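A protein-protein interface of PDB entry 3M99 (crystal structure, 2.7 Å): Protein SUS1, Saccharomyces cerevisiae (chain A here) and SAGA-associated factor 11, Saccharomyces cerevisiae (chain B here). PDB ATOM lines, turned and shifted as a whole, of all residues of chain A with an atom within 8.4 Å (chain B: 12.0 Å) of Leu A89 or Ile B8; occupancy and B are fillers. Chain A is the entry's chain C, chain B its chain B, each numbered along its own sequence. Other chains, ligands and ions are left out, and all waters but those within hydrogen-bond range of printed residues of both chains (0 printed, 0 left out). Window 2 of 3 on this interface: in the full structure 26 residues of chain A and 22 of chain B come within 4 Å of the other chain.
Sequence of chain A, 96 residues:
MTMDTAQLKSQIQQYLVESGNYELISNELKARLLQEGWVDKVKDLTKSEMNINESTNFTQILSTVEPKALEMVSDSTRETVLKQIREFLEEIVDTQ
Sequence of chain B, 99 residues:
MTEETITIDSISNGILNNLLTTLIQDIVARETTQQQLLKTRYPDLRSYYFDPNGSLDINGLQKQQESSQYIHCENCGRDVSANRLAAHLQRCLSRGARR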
ATOM      1  N   LYS A   9      34.558 -21.919 -13.979  1.00  0.00           N
ATOM      2  CA  LYS A   9      33.798 -21.125 -13.022  1.00  0.00           C
ATOM      3  C   LYS A   9      33.768 -19.668 -13.471  1.00  0.00           C
ATOM      4  O   LYS A   9      32.810 -18.939 -13.198  1.00  0.00           O
ATOM      5  CB  LYS A   9      34.410 -21.239 -11.625  1.00  0.00           C
ATOM      6  CG  LYS A   9      33.872 -20.232 -10.610  1.00  0.00           C
ATOM      7  CD  LYS A   9      32.373 -20.388 -10.385  1.00  0.00           C
ATOM      8  CE  LYS A   9      31.912 -19.613  -9.156  1.00  0.00           C
ATOM      9  NZ  LYS A   9      32.218 -18.160  -9.256  1.00  0.00           N
ATOM     10  N   ILE A  12      31.740 -19.544 -17.099  1.00  0.00           N
ATOM     11  CA  ILE A  12      30.300 -19.630 -16.909  1.00  0.00           C
ATOM     12  C   ILE A  12      29.756 -18.292 -16.396  1.00  0.00           C
ATOM     13  O   ILE A  12      28.589 -17.953 -16.601  1.00  0.00           O
ATOM     14  CB  ILE A  12      29.941 -20.793 -15.958  1.00  0.00           C
ATOM     15  CG1 ILE A  12      28.428 -21.005 -15.895  1.00  0.00           C
ATOM     16  CG2 ILE A  12      30.507 -20.545 -14.569  1.00  0.00           C
ATOM     17  CD1 ILE A  12      27.738 -20.169 -14.834  1.00  0.00           C
ATOM     18  N   GLN A  13      30.624 -17.526 -15.744  1.00  0.00           N
ATOM     19  CA  GLN A  13      30.275 -16.200 -15.260  1.00  0.00           C
ATOM     20  C   GLN A  13      30.330 -15.240 -16.441  1.00  0.00           C
ATOM     21  O   GLN A  13      29.556 -14.291 -16.528  1.00  0.00           O
ATOM     22  CB  GLN A  13      31.275 -15.773 -14.185  1.00  0.00           C
ATOM     23  CG  GLN A  13      30.676 -15.090 -12.968  1.00  0.00           C
ATOM     24  CD  GLN A  13      31.688 -14.948 -11.838  1.00  0.00           C
ATOM     25  OE1 GLN A  13      31.534 -14.117 -10.946  1.00  0.00           O
ATOM     26  NE2 GLN A  13      32.736 -15.763 -11.880  1.00  0.00           N
ATOM     27  N   TYR A  15      29.525 -15.784 -19.591  1.00  0.00           N
ATOM     28  CA  TYR A  15      28.320 -15.824 -20.410  1.00  0.00           C
ATOM     29  C   TYR A  15      27.249 -14.933 -19.809  1.00  0.00           C
ATOM     30  O   TYR A  15      26.700 -14.068 -20.488  1.00  0.00           O
ATOM     31  CB  TYR A  15      27.769 -17.242 -20.557  1.00  0.00           C
ATOM     32  CG  TYR A  15      26.374 -17.255 -21.147  1.00  0.00           C
ATOM     33  CD1 TYR A  15      25.249 -17.271 -20.329  1.00  0.00           C
ATOM     34  CD2 TYR A  15      26.179 -17.219 -22.525  1.00  0.00           C
ATOM     35  CE1 TYR A  15      23.962 -17.266 -20.866  1.00  0.00           C
ATOM     36  CE2 TYR A  15      24.897 -17.214 -23.073  1.00  0.00           C
ATOM     37  CZ  TYR A  15      23.792 -17.239 -22.239  1.00  0.00           C
ATOM     38  OH  TYR A  15      22.521 -17.235 -22.777  1.00  0.00           O
ATOM     39  N   LEU A  16      26.953 -15.154 -18.533  1.00  0.00           N
ATOM     40  CA  LEU A  16      25.923 -14.381 -17.853  1.00  0.00           C
ATOM     41  C   LEU A  16      26.030 -12.893 -18.175  1.00  0.00           C
ATOM     42  O   LEU A  16      25.026 -12.237 -18.444  1.00  0.00           O
ATOM     43  CB  LEU A  16      25.965 -14.620 -16.340  1.00  0.00           C
ATOM     44  CG  LEU A  16      24.959 -15.636 -15.793  1.00  0.00           C
ATOM     45  CD1 LEU A  16      24.928 -16.896 -16.635  1.00  0.00           C
ATOM     46  CD2 LEU A  16      25.274 -15.965 -14.353  1.00  0.00           C
ATOM     47  N   ASN A  21      22.302 -11.228 -18.738  1.00  0.00           N
ATOM     48  CA  ASN A  21      21.606 -11.939 -17.673  1.00  0.00           C
ATOM     49  C   ASN A  21      22.256 -11.750 -16.312  1.00  0.00           C
ATOM     50  O   ASN A  21      21.698 -12.136 -15.287  1.00  0.00           O
ATOM     51  CB  ASN A  21      21.497 -13.426 -17.992  1.00  0.00           C
ATOM     52  CG  ASN A  21      20.279 -13.750 -18.825  1.00  0.00           C
ATOM     53  OD1 ASN A  21      19.935 -13.021 -19.759  1.00  0.00           O
ATOM     54  ND2 ASN A  21      19.612 -14.850 -18.491  1.00  0.00           N
ATOM     55  N   ILE A  25      20.310 -10.159 -12.726  1.00  0.00           N
ATOM     56  CA  ILE A  25      20.303 -10.815 -11.423  1.00  0.00           C
ATOM     57  C   ILE A  25      20.778  -9.894 -10.315  1.00  0.00           C
ATOM     58  O   ILE A  25      20.300  -9.981  -9.185  1.00  0.00           O
ATOM     59  CB  ILE A  25      21.152 -12.082 -11.419  1.00  0.00           C
ATOM     60  CG1 ILE A  25      20.637 -13.053 -12.477  1.00  0.00           C
ATOM     61  CG2 ILE A  25      21.107 -12.733 -10.052  1.00  0.00           C
ATOM     62  CD1 ILE A  25      21.594 -14.169 -12.789  1.00  0.00           C
ATOM     63  N   LEU A  82      18.341 -17.220  -5.925  1.00  0.00           N
ATOM     64  CA  LEU A  82      19.195 -18.360  -6.226  1.00  0.00           C
ATOM     65  C   LEU A  82      18.503 -19.244  -7.262  1.00  0.00           C
ATOM     66  O   LEU A  82      19.137 -19.766  -8.180  1.00  0.00           O
ATOM     67  CB  LEU A  82      19.494 -19.148  -4.952  1.00  0.00           C
ATOM     68  CG  LEU A  82      20.814 -19.918  -4.901  1.00  0.00           C
ATOM     69  CD1 LEU A  82      22.000 -18.982  -5.074  1.00  0.00           C
ATOM     70  CD2 LEU A  82      20.921 -20.678  -3.594  1.00  0.00           C
ATOM     71  N   LYS A  83      17.190 -19.391  -7.113  1.00  0.00           N
ATOM     72  CA  LYS A  83      16.373 -20.188  -8.021  1.00  0.00           C
ATOM     73  C   LYS A  83      16.418 -19.578  -9.415  1.00  0.00           C
ATOM     74  O   LYS A  83      16.408 -20.285 -10.422  1.00  0.00           O
ATOM     75  CB  LYS A  83      14.926 -20.216  -7.517  1.00  0.00           C
ATOM     76  CG  LYS A  83      14.291 -21.599  -7.433  1.00  0.00           C
ATOM     77  CD  LYS A  83      13.588 -21.993  -8.718  1.00  0.00           C
ATOM     78  CE  LYS A  83      12.796 -23.276  -8.516  1.00  0.00           C
ATOM     79  NZ  LYS A  83      12.160 -23.757  -9.773  1.00  0.00           N
ATOM     80  N   GLN A  84      16.458 -18.251  -9.455  1.00  0.00           N
ATOM     81  CA  GLN A  84      16.582 -17.508 -10.700  1.00  0.00           C
ATOM     82  C   GLN A  84      17.938 -17.785 -11.344  1.00  0.00           C
ATOM     83  O   GLN A  84      18.031 -17.985 -12.557  1.00  0.00           O
ATOM     84  CB  GLN A  84      16.423 -16.013 -10.423  1.00  0.00           C
ATOM     85  CG  GLN A  84      16.486 -15.124 -11.649  1.00  0.00           C
ATOM     86  CD  GLN A  84      16.651 -13.664 -11.280  1.00  0.00           C
ATOM     87  OE1 GLN A  84      16.175 -12.772 -11.981  1.00  0.00           O
ATOM     88  NE2 GLN A  84      17.325 -13.414 -10.165  1.00  0.00           N
ATOM     89  N   ILE A  85      18.986 -17.794 -10.522  1.00  0.00           N
ATOM     90  CA  ILE A  85      20.332 -18.108 -10.988  1.00  0.00           C
ATOM     91  C   ILE A  85      20.355 -19.469 -11.667  1.00  0.00           C
ATOM     92  O   ILE A  85      20.852 -19.610 -12.783  1.00  0.00           O
ATOM     93  CB  ILE A  85      21.340 -18.155  -9.823  1.00  0.00           C
ATOM     94  CG1 ILE A  85      21.493 -16.780  -9.177  1.00  0.00           C
ATOM     95  CG2 ILE A  85      22.687 -18.666 -10.307  1.00  0.00           C
ATOM     96  CD1 ILE A  85      22.434 -15.872  -9.911  1.00  0.00           C
ATOM     97  N   ARG A  86      19.808 -20.467 -10.979  1.00  0.00           N
ATOM     98  CA  ARG A  86      19.851 -21.851 -11.438  1.00  0.00           C
ATOM     99  C   ARG A  86      19.321 -22.027 -12.858  1.00  0.00           C
ATOM    100  O   ARG A  86      20.001 -22.586 -13.719  1.00  0.00           O
ATOM    101  CB  ARG A  86      19.089 -22.757 -10.464  1.00  0.00           C
ATOM    102  CG  ARG A  86      19.709 -22.802  -9.074  1.00  0.00           C
ATOM    103  CD  ARG A  86      19.033 -23.817  -8.156  1.00  0.00           C
ATOM    104  NE  ARG A  86      19.847 -24.081  -6.968  1.00  0.00           N
ATOM    105  CZ  ARG A  86      19.652 -23.517  -5.777  1.00  0.00           C
ATOM    106  NH1 ARG A  86      18.656 -22.657  -5.599  1.00  0.00           N
ATOM    107  NH2 ARG A  86      20.452 -23.819  -4.762  1.00  0.00           N
ATOM    108  N   GLU A  87      18.110 -21.542 -13.099  1.00  0.00           N
ATOM    109  CA  GLU A  87      17.459 -21.743 -14.385  1.00  0.00           C
ATOM    110  C   GLU A  87      18.182 -21.027 -15.528  1.00  0.00           C
ATOM    111  O   GLU A  87      17.807 -21.166 -16.694  1.00  0.00           O
ATOM    112  CB  GLU A  87      16.002 -21.297 -14.307  1.00  0.00           C
ATOM    113  CG  GLU A  87      15.196 -21.622 -15.541  1.00  0.00           C
ATOM    114  CD  GLU A  87      13.764 -21.175 -15.414  1.00  0.00           C
ATOM    115  OE1 GLU A  87      13.211 -21.287 -14.300  1.00  0.00           O
ATOM    116  OE2 GLU A  87      13.195 -20.712 -16.425  1.00  0.00           O
ATOM    117  N   PHE A  88      19.217 -20.265 -15.189  1.00  0.00           N
ATOM    118  CA  PHE A  88      20.069 -19.631 -16.195  1.00  0.00           C
ATOM    119  C   PHE A  88      21.276 -20.505 -16.530  1.00  0.00           C
ATOM    120  O   PHE A  88      21.713 -20.569 -17.680  1.00  0.00           O
ATOM    121  CB  PHE A  88      20.550 -18.253 -15.730  1.00  0.00           C
ATOM    122  CG  PHE A  88      19.514 -17.175 -15.844  1.00  0.00           C
ATOM    123  CD1 PHE A  88      19.545 -16.080 -14.998  1.00  0.00           C
ATOM    124  CD2 PHE A  88      18.506 -17.257 -16.792  1.00  0.00           C
ATOM    125  CE1 PHE A  88      18.600 -15.083 -15.097  1.00  0.00           C
ATOM    126  CE2 PHE A  88      17.549 -16.263 -16.895  1.00  0.00           C
ATOM    127  CZ  PHE A  88      17.598 -15.175 -16.047  1.00  0.00           C
ATOM    128  N   LEU A  89      21.817 -21.170 -15.516  1.00  0.00           N
ATOM    129  CA  LEU A  89      22.966 -22.042 -15.710  1.00  0.00           C
ATOM    130  C   LEU A  89      22.597 -23.198 -16.629  1.00  0.00           C
ATOM    131  O   LEU A  89      23.397 -23.617 -17.466  1.00  0.00           O
ATOM    132  CB  LEU A  89      23.477 -22.571 -14.366  1.00  0.00           C
ATOM    133  CG  LEU A  89      24.442 -21.685 -13.571  1.00  0.00           C
ATOM    134  CD1 LEU A  89      23.979 -20.239 -13.535  1.00  0.00           C
ATOM    135  CD2 LEU A  89      24.631 -22.226 -12.159  1.00  0.00           C
ATOM    136  N   GLU A  90      21.376 -23.703 -16.478  1.00  0.00           N
ATOM    137  CA  GLU A  90      20.906 -24.827 -17.281  1.00  0.00           C
ATOM    138  C   GLU A  90      20.636 -24.392 -18.722  1.00  0.00           C
ATOM    139  O   GLU A  90      20.196 -25.183 -19.555  1.00  0.00           O
ATOM    140  CB  GLU A  90      19.664 -25.460 -16.646  1.00  0.00           C
ATOM    141  CG  GLU A  90      19.815 -25.722 -15.149  1.00  0.00           C
ATOM    142  CD  GLU A  90      18.829 -26.747 -14.613  1.00  0.00           C
ATOM    143  OE1 GLU A  90      18.951 -27.937 -14.975  1.00  0.00           O
ATOM    144  OE2 GLU A  90      17.947 -26.362 -13.814  1.00  0.00           O
ATOM    145  N   GLU A  91      20.911 -23.123 -19.001  1.00  0.00           N
ATOM    146  CA  GLU A  91      20.819 -22.598 -20.352  1.00  0.00           C
ATOM    147  C   GLU A  91      22.162 -22.743 -21.047  1.00  0.00           C
ATOM    148  O   GLU A  91      22.255 -22.640 -22.270  1.00  0.00           O
ATOM    149  CB  GLU A  91      20.420 -21.122 -20.325  1.00  0.00           C
ATOM    150  CG  GLU A  91      19.070 -20.843 -19.692  1.00  0.00           C
ATOM    151  CD  GLU A  91      17.912 -21.290 -20.560  1.00  0.00           C
ATOM    152  OE1 GLU A  91      17.950 -22.429 -21.078  1.00  0.00           O
ATOM    153  OE2 GLU A  91      16.958 -20.501 -20.716  1.00  0.00           O
ATOM    154  N   ILE A  92      23.208 -22.979 -20.260  1.00  0.00           N
ATOM    155  CA  ILE A  92      24.561 -23.025 -20.801  1.00  0.00           C
ATOM    156  C   ILE A  92      25.408 -24.148 -20.205  1.00  0.00           C
ATOM    157  O   ILE A  92      26.635 -24.137 -20.313  1.00  0.00           O
ATOM    158  CB  ILE A  92      25.289 -21.678 -20.601  1.00  0.00           C
ATOM    159  CG1 ILE A  92      25.479 -21.381 -19.113  1.00  0.00           C
ATOM    160  CG2 ILE A  92      24.515 -20.551 -21.260  1.00  0.00           C
ATOM    161  CD1 ILE A  92      26.226 -20.089 -18.840  1.00  0.00           C
ATOM    162  N   VAL A  93      24.753 -25.122 -19.584  1.00  0.00           N
ATOM    163  CA  VAL A  93      25.478 -26.212 -18.945  1.00  0.00           C
ATOM    164  C   VAL A  93      24.842 -27.576 -19.192  1.00  0.00           C
ATOM    165  O   VAL A  93      23.663 -27.787 -18.897  1.00  0.00           O
ATOM    166  CB  VAL A  93      25.612 -25.985 -17.423  1.00  0.00           C
ATOM    167  CG1 VAL A  93      26.256 -27.193 -16.755  1.00  0.00           C
ATOM    168  CG2 VAL A  93      26.417 -24.724 -17.145  1.00  0.00           C
ATOM    169  N   ASP A  94      25.633 -28.493 -19.742  1.00  0.00           N
ATOM    170  CA  ASP A  94      25.226 -29.887 -19.848  1.00  0.00           C
ATOM    171  C   ASP A  94      25.316 -30.520 -18.465  1.00  0.00           C
ATOM    172  O   ASP A  94      26.267 -30.272 -17.723  1.00  0.00           O
ATOM    173  CB  ASP A  94      26.111 -30.638 -20.847  1.00  0.00           C
ATOM    174  CG  ASP A  94      25.748 -30.337 -22.292  1.00  0.00           C
ATOM    175  OD1 ASP A  94      24.612 -30.655 -22.702  1.00  0.00           O
ATOM    176  OD2 ASP A  94      26.602 -29.791 -23.023  1.00  0.00           O
ATOM    177  N   THR A  95      24.318 -31.326 -18.121  1.00  0.00           N
ATOM    178  CA  THR A  95      24.216 -31.905 -16.783  1.00  0.00           C
ATOM    179  C   THR A  95      25.446 -32.736 -16.397  1.00  0.00           C
ATOM    180  O   THR A  95      26.534 -32.192 -16.204  1.00  0.00           O
ATOM    181  CB  THR A  95      22.907 -32.728 -16.621  1.00  0.00           C
ATOM    182  OG1 THR A  95      22.913 -33.422 -15.366  1.00  0.00           O
ATOM    183  CG2 THR A  95      22.735 -33.723 -17.767  1.00  0.00           C
ATOM    184  N   GLN A  96      25.263 -34.048 -16.279  1.00  0.00           N
ATOM    185  CA  GLN A  96      26.340 -34.946 -15.872  1.00  0.00           C
ATOM    186  C   GLN A  96      26.854 -34.625 -14.468  1.00  0.00           C
ATOM    187  O   GLN A  96      26.639 -35.394 -13.528  1.00  0.00           O
ATOM    188  CB  GLN A  96      27.485 -34.917 -16.892  1.00  0.00           C
ATOM    189  CG  GLN A  96      27.226 -35.744 -18.148  1.00  0.00           C
ATOM    190  CD  GLN A  96      25.939 -35.361 -18.855  1.00  0.00           C
ATOM    191  OE1 GLN A  96      25.705 -34.191 -19.156  1.00  0.00           O
ATOM    192  NE2 GLN A  96      25.099 -36.353 -19.126  1.00  0.00           N
ATOM    193  OXT GLN A  96      27.487 -33.593 -14.233  1.00  0.00           O
ATOM    194  N   THR B   7      27.576 -29.375  -7.788  1.00  0.00           N
ATOM    195  CA  THR B   7      28.272 -28.415  -8.637  1.00  0.00           C
ATOM    196  C   THR B   7      27.277 -27.592  -9.463  1.00  0.00           C
ATOM    197  O   THR B   7      27.650 -26.606 -10.096  1.00  0.00           O
ATOM    198  CB  THR B   7      29.328 -29.105  -9.551  1.00  0.00           C
ATOM    199  OG1 THR B   7      30.279 -29.812  -8.745  1.00  0.00           O
ATOM    200  CG2 THR B   7      30.077 -28.084 -10.395  1.00  0.00           C
ATOM    201  N   ILE B   8      26.007 -27.997  -9.452  1.00  0.00           N
ATOM    202  CA  ILE B   8      24.954 -27.185 -10.057  1.00  0.00           C
ATOM    203  C   ILE B   8      24.572 -26.091  -9.073  1.00  0.00           C
ATOM    204  O   ILE B   8      24.109 -25.016  -9.456  1.00  0.00           O
ATOM    205  CB  ILE B   8      23.681 -28.002 -10.384  1.00  0.00           C
ATOM    206  CG1 ILE B   8      24.032 -29.369 -10.972  1.00  0.00           C
ATOM    207  CG2 ILE B   8      22.786 -27.224 -11.335  1.00  0.00           C
ATOM    208  CD1 ILE B   8      22.820 -30.211 -11.311  1.00  0.00           C
ATOM    209  N   ASP B   9      24.776 -26.389  -7.794  1.00  0.00           N
ATOM    210  CA  ASP B   9      24.410 -25.492  -6.709  1.00  0.00           C
ATOM    211  C   ASP B   9      25.647 -24.803  -6.171  1.00  0.00           C
ATOM    212  O   ASP B   9      25.598 -23.653  -5.734  1.00  0.00           O
ATOM    213  CB  ASP B   9      23.750 -26.279  -5.578  1.00  0.00           C
ATOM    214  CG  ASP B   9      22.837 -27.370  -6.087  1.00  0.00           C
ATOM    215  OD1 ASP B   9      23.352 -28.405  -6.569  1.00  0.00           O
ATOM    216  OD2 ASP B   9      21.602 -27.195  -5.997  1.00  0.00           O
ATOM    217  N   SER B  10      26.760 -25.523  -6.192  1.00  0.00           N
ATOM    218  CA  SER B  10      28.023 -24.955  -5.765  1.00  0.00           C
ATOM    219  C   SER B  10      28.284 -23.659  -6.527  1.00  0.00           C
ATOM    220  O   SER B  10      28.755 -22.678  -5.954  1.00  0.00           O
ATOM    221  CB  SER B  10      29.157 -25.956  -5.993  1.00  0.00           C
ATOM    222  OG  SER B  10      28.872 -27.198  -5.371  1.00  0.00           O
ATOM    223  N   ILE B  11      27.961 -23.652  -7.817  1.00  0.00           N
ATOM    224  CA  ILE B  11      28.196 -22.477  -8.649  1.00  0.00           C
ATOM    225  C   ILE B  11      27.223 -21.364  -8.304  1.00  0.00           C
ATOM    226  O   ILE B  11      27.604 -20.198  -8.229  1.00  0.00           O
ATOM    227  CB  ILE B  11      28.058 -22.789 -10.149  1.00  0.00           C
ATOM    228  CG1 ILE B  11      29.056 -23.870 -10.576  1.00  0.00           C
ATOM    229  CG2 ILE B  11      28.256 -21.522 -10.970  1.00  0.00           C
ATOM    230  CD1 ILE B  11      30.508 -23.450 -10.481  1.00  0.00           C
ATOM    231  N   SER B  12      25.963 -21.733  -8.103  1.00  0.00           N
ATOM    232  CA  SER B  12      24.926 -20.778  -7.738  1.00  0.00           C
ATOM    233  C   SER B  12      25.264 -20.065  -6.430  1.00  0.00           C
ATOM    234  O   SER B  12      25.401 -18.843  -6.402  1.00  0.00           O
ATOM    235  CB  SER B  12      23.570 -21.475  -7.628  1.00  0.00           C
ATOM    236  OG  SER B  12      23.086 -21.855  -8.905  1.00  0.00           O
ATOM    237  N   ASN B  13      25.404 -20.824  -5.348  1.00  0.00           N
ATOM    238  CA  ASN B  13      25.719 -20.223  -4.055  1.00  0.00           C
ATOM    239  C   ASN B  13      27.007 -19.410  -4.098  1.00  0.00           C
ATOM    240  O   ASN B  13      27.208 -18.493  -3.299  1.00  0.00           O
ATOM    241  CB  ASN B  13      25.767 -21.281  -2.950  1.00  0.00           C
ATOM    242  CG  ASN B  13      24.401 -21.546  -2.343  1.00  0.00           C
ATOM    243  OD1 ASN B  13      23.806 -20.665  -1.718  1.00  0.00           O
ATOM    244  ND2 ASN B  13      23.897 -22.762  -2.523  1.00  0.00           N
ATOM    245  N   GLY B  14      27.874 -19.744  -5.044  1.00  0.00           N
ATOM    246  CA  GLY B  14      29.074 -18.965  -5.266  1.00  0.00           C
ATOM    247  C   GLY B  14      28.704 -17.628  -5.869  1.00  0.00           C
ATOM    248  O   GLY B  14      29.016 -16.577  -5.305  1.00  0.00           O
ATOM    249  N   ILE B  15      28.024 -17.681  -7.015  1.00  0.00           N
ATOM    250  CA  ILE B  15      27.555 -16.489  -7.721  1.00  0.00           C
ATOM    251  C   ILE B  15      26.778 -15.562  -6.799  1.00  0.00           C
ATOM    252  O   ILE B  15      26.898 -14.341  -6.885  1.00  0.00           O
ATOM    253  CB  ILE B  15      26.641 -16.855  -8.903  1.00  0.00           C
ATOM    254  CG1 ILE B  15      27.372 -17.760  -9.899  1.00  0.00           C
ATOM    255  CG2 ILE B  15      26.145 -15.597  -9.588  1.00  0.00           C
ATOM    256  CD1 ILE B  15      28.431 -17.052 -10.717  1.00  0.00           C
ATOM    257  N   LEU B  16      25.980 -16.152  -5.919  1.00  0.00           N
ATOM    258  CA  LEU B  16      25.208 -15.376  -4.967  1.00  0.00           C
ATOM    259  C   LEU B  16      26.125 -14.740  -3.929  1.00  0.00           C
ATOM    260  O   LEU B  16      26.073 -13.530  -3.720  1.00  0.00           O
ATOM    261  CB  LEU B  16      24.154 -16.249  -4.287  1.00  0.00           C
ATOM    262  CG  LEU B  16      23.033 -15.490  -3.581  1.00  0.00           C
ATOM    263  CD1 LEU B  16      22.169 -14.795  -4.612  1.00  0.00           C
ATOM    264  CD2 LEU B  16      22.198 -16.418  -2.712  1.00  0.00           C
ATOM    265  N   ASN B  17      26.968 -15.553  -3.290  1.00  0.00           N
ATOM    266  CA  ASN B  17      27.875 -15.053  -2.256  1.00  0.00           C
ATOM    267  C   ASN B  17      28.754 -13.943  -2.807  1.00  0.00           C
ATOM    268  O   ASN B  17      29.149 -13.035  -2.082  1.00  0.00           O
ATOM    269  CB  ASN B  17      28.744 -16.179  -1.685  1.00  0.00           C
ATOM    270  CG  ASN B  17      29.737 -15.685  -0.631  1.00  0.00           C
ATOM    271  OD1 ASN B  17      29.346 -15.162   0.415  1.00  0.00           O
ATOM    272  ND2 ASN B  17      31.029 -15.863  -0.903  1.00  0.00           N
ATOM    273  N   ASN B  18      29.051 -14.025  -4.097  1.00  0.00           N
ATOM    274  CA  ASN B  18      29.869 -13.020  -4.759  1.00  0.00           C
ATOM    275  C   ASN B  18      29.157 -11.686  -4.842  1.00  0.00           C
ATOM    276  O   ASN B  18      29.711 -10.654  -4.466  1.00  0.00           O
ATOM    277  CB  ASN B  18      30.235 -13.480  -6.163  1.00  0.00           C
ATOM    278  CG  ASN B  18      31.442 -14.377  -6.182  1.00  0.00           C
ATOM    279  OD1 ASN B  18      31.576 -15.278  -5.357  1.00  0.00           O
ATOM    280  ND2 ASN B  18      32.331 -14.137  -7.131  1.00  0.00           N
ATOM    281  N   LEU B  19      27.927 -11.722  -5.351  1.00  0.00           N
ATOM    282  CA  LEU B  19      27.068 -10.542  -5.418  1.00  0.00           C
ATOM    283  C   LEU B  19      26.813  -9.978  -4.022  1.00  0.00           C
ATOM    284  O   LEU B  19      26.839  -8.767  -3.820  1.00  0.00           O
ATOM    285  CB  LEU B  19      25.736 -10.889  -6.092  1.00  0.00           C
ATOM    286  CG  LEU B  19      25.773 -11.265  -7.576  1.00  0.00           C
ATOM    287  CD1 LEU B  19      24.503 -11.994  -7.990  1.00  0.00           C
ATOM    288  CD2 LEU B  19      26.000 -10.034  -8.441  1.00  0.00           C
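CD1 of Ile B11 touches CD of Lys A9 (3.6 Å).
Gln A13 touches Asn B18 (OE1 to ND2, 3.9 Å).
Ser B12 touches Leu A82 (O to CD1, 3.7 Å).
Leu A82 touches Asn B13.
Ser B12 touches Ile A85 (OG to CG2, 3.5 Å).
CG2 of Ile B15 touches CD1 of Ile A85, 3.7 Å away.
Ser B12 touches Arg A86 (OG to CG, 3.5 Å).
CD2 of Leu A89 touches O of Ile B8, at 3.9 Å.
Ile B11 touches Leu A89 (CG2 to CD2, 3.9 Å).
Ser B12 touches Leu A89.
Printed residues of chain B that touch a printed residue of chain A: Ile B8, Asp B9, Ile B11, Ser B12, Asn B13, Ile B15, Leu B16 and Asn B18.
Hydrophobic or aromatic side chains of chain B that line the printed part of chain A: Ile B11, Ile B15 and Leu B16.
Of the 22 printed residues of chain A, 6 touch a printed residue of chain B.
Hydrophobic or aromatic side chains of chain A within 4 Å of the printed part of chain B: Leu A82, Ile A85 and Leu A89.
Among the printed residues, 13 pairs touch across the chains.
Among the printed residues, Asp or Glu carboxylates within 4 Å of a Lys or Arg side-chain nitrogen of the other chain: Arg A86 with Asp B9 (3.7 Å).
Leu A89 touches just these residues of chain B: Ile B8 (3.9 Å), Ile B11 (3.9 Å) and Ser B12 (3.6 Å).
Printed residues of chain B within 4 Å of Arg A86: Asp B9 and Ser B12.
No residue of chain B comes within 4 Å of Phe A88.
No residue of chain B comes within 4 Å of Glu A90.
No residue of chain B comes within 4 Å of Ile A92.
No residue of chain B comes within 4 Å of Val A93.
Of the printed residues of chain A, Asn B18 touches Gln A13.
Of the printed residues of chain A, Ile B15 touches Gln A13 (3.7 Å) and Ile A85 (3.7 Å).
Printed residues of chain A within 4 Å of Ser B12: Leu A82 (3.7 Å), Ile A85 (3.5 Å), Arg A86 (3.5 Å) and Leu A89 (3.6 Å).
Printed residues of chain A within 4 Å of Asp B9: Arg A86.
Of the printed residues of chain B, Lys A9 touches Ile B11.
Ile A12 touches none of the printed residues of chain B.
The nearest residue of chain A that does not touch Ile B8 is Arg A86 (4.9 Å).
The nearest printed residue of chain A that does not touch Asn B18 is Lys A9 (4.6 Å).
The backbone carbonyl oxygen of Lys A9 lies within hydrogen-bond range of the side-chain amide nitrogen of Gln A13, at 3.4 Å.
O of Ile B8 lies within hydrogen-bond range of OG of Ser B12, at 3.4 Å.
The side-chain amide oxygen (OD1) of Asn B18 lies close to the backbone carbonyl oxygen (O) of Gly B14 (2.9 Å).
The side-chain carboxylate (OD2) of Asp B9 lies within salt-bridge range of the guanidinium group (NE) of Arg A86, 3.7 Å away.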
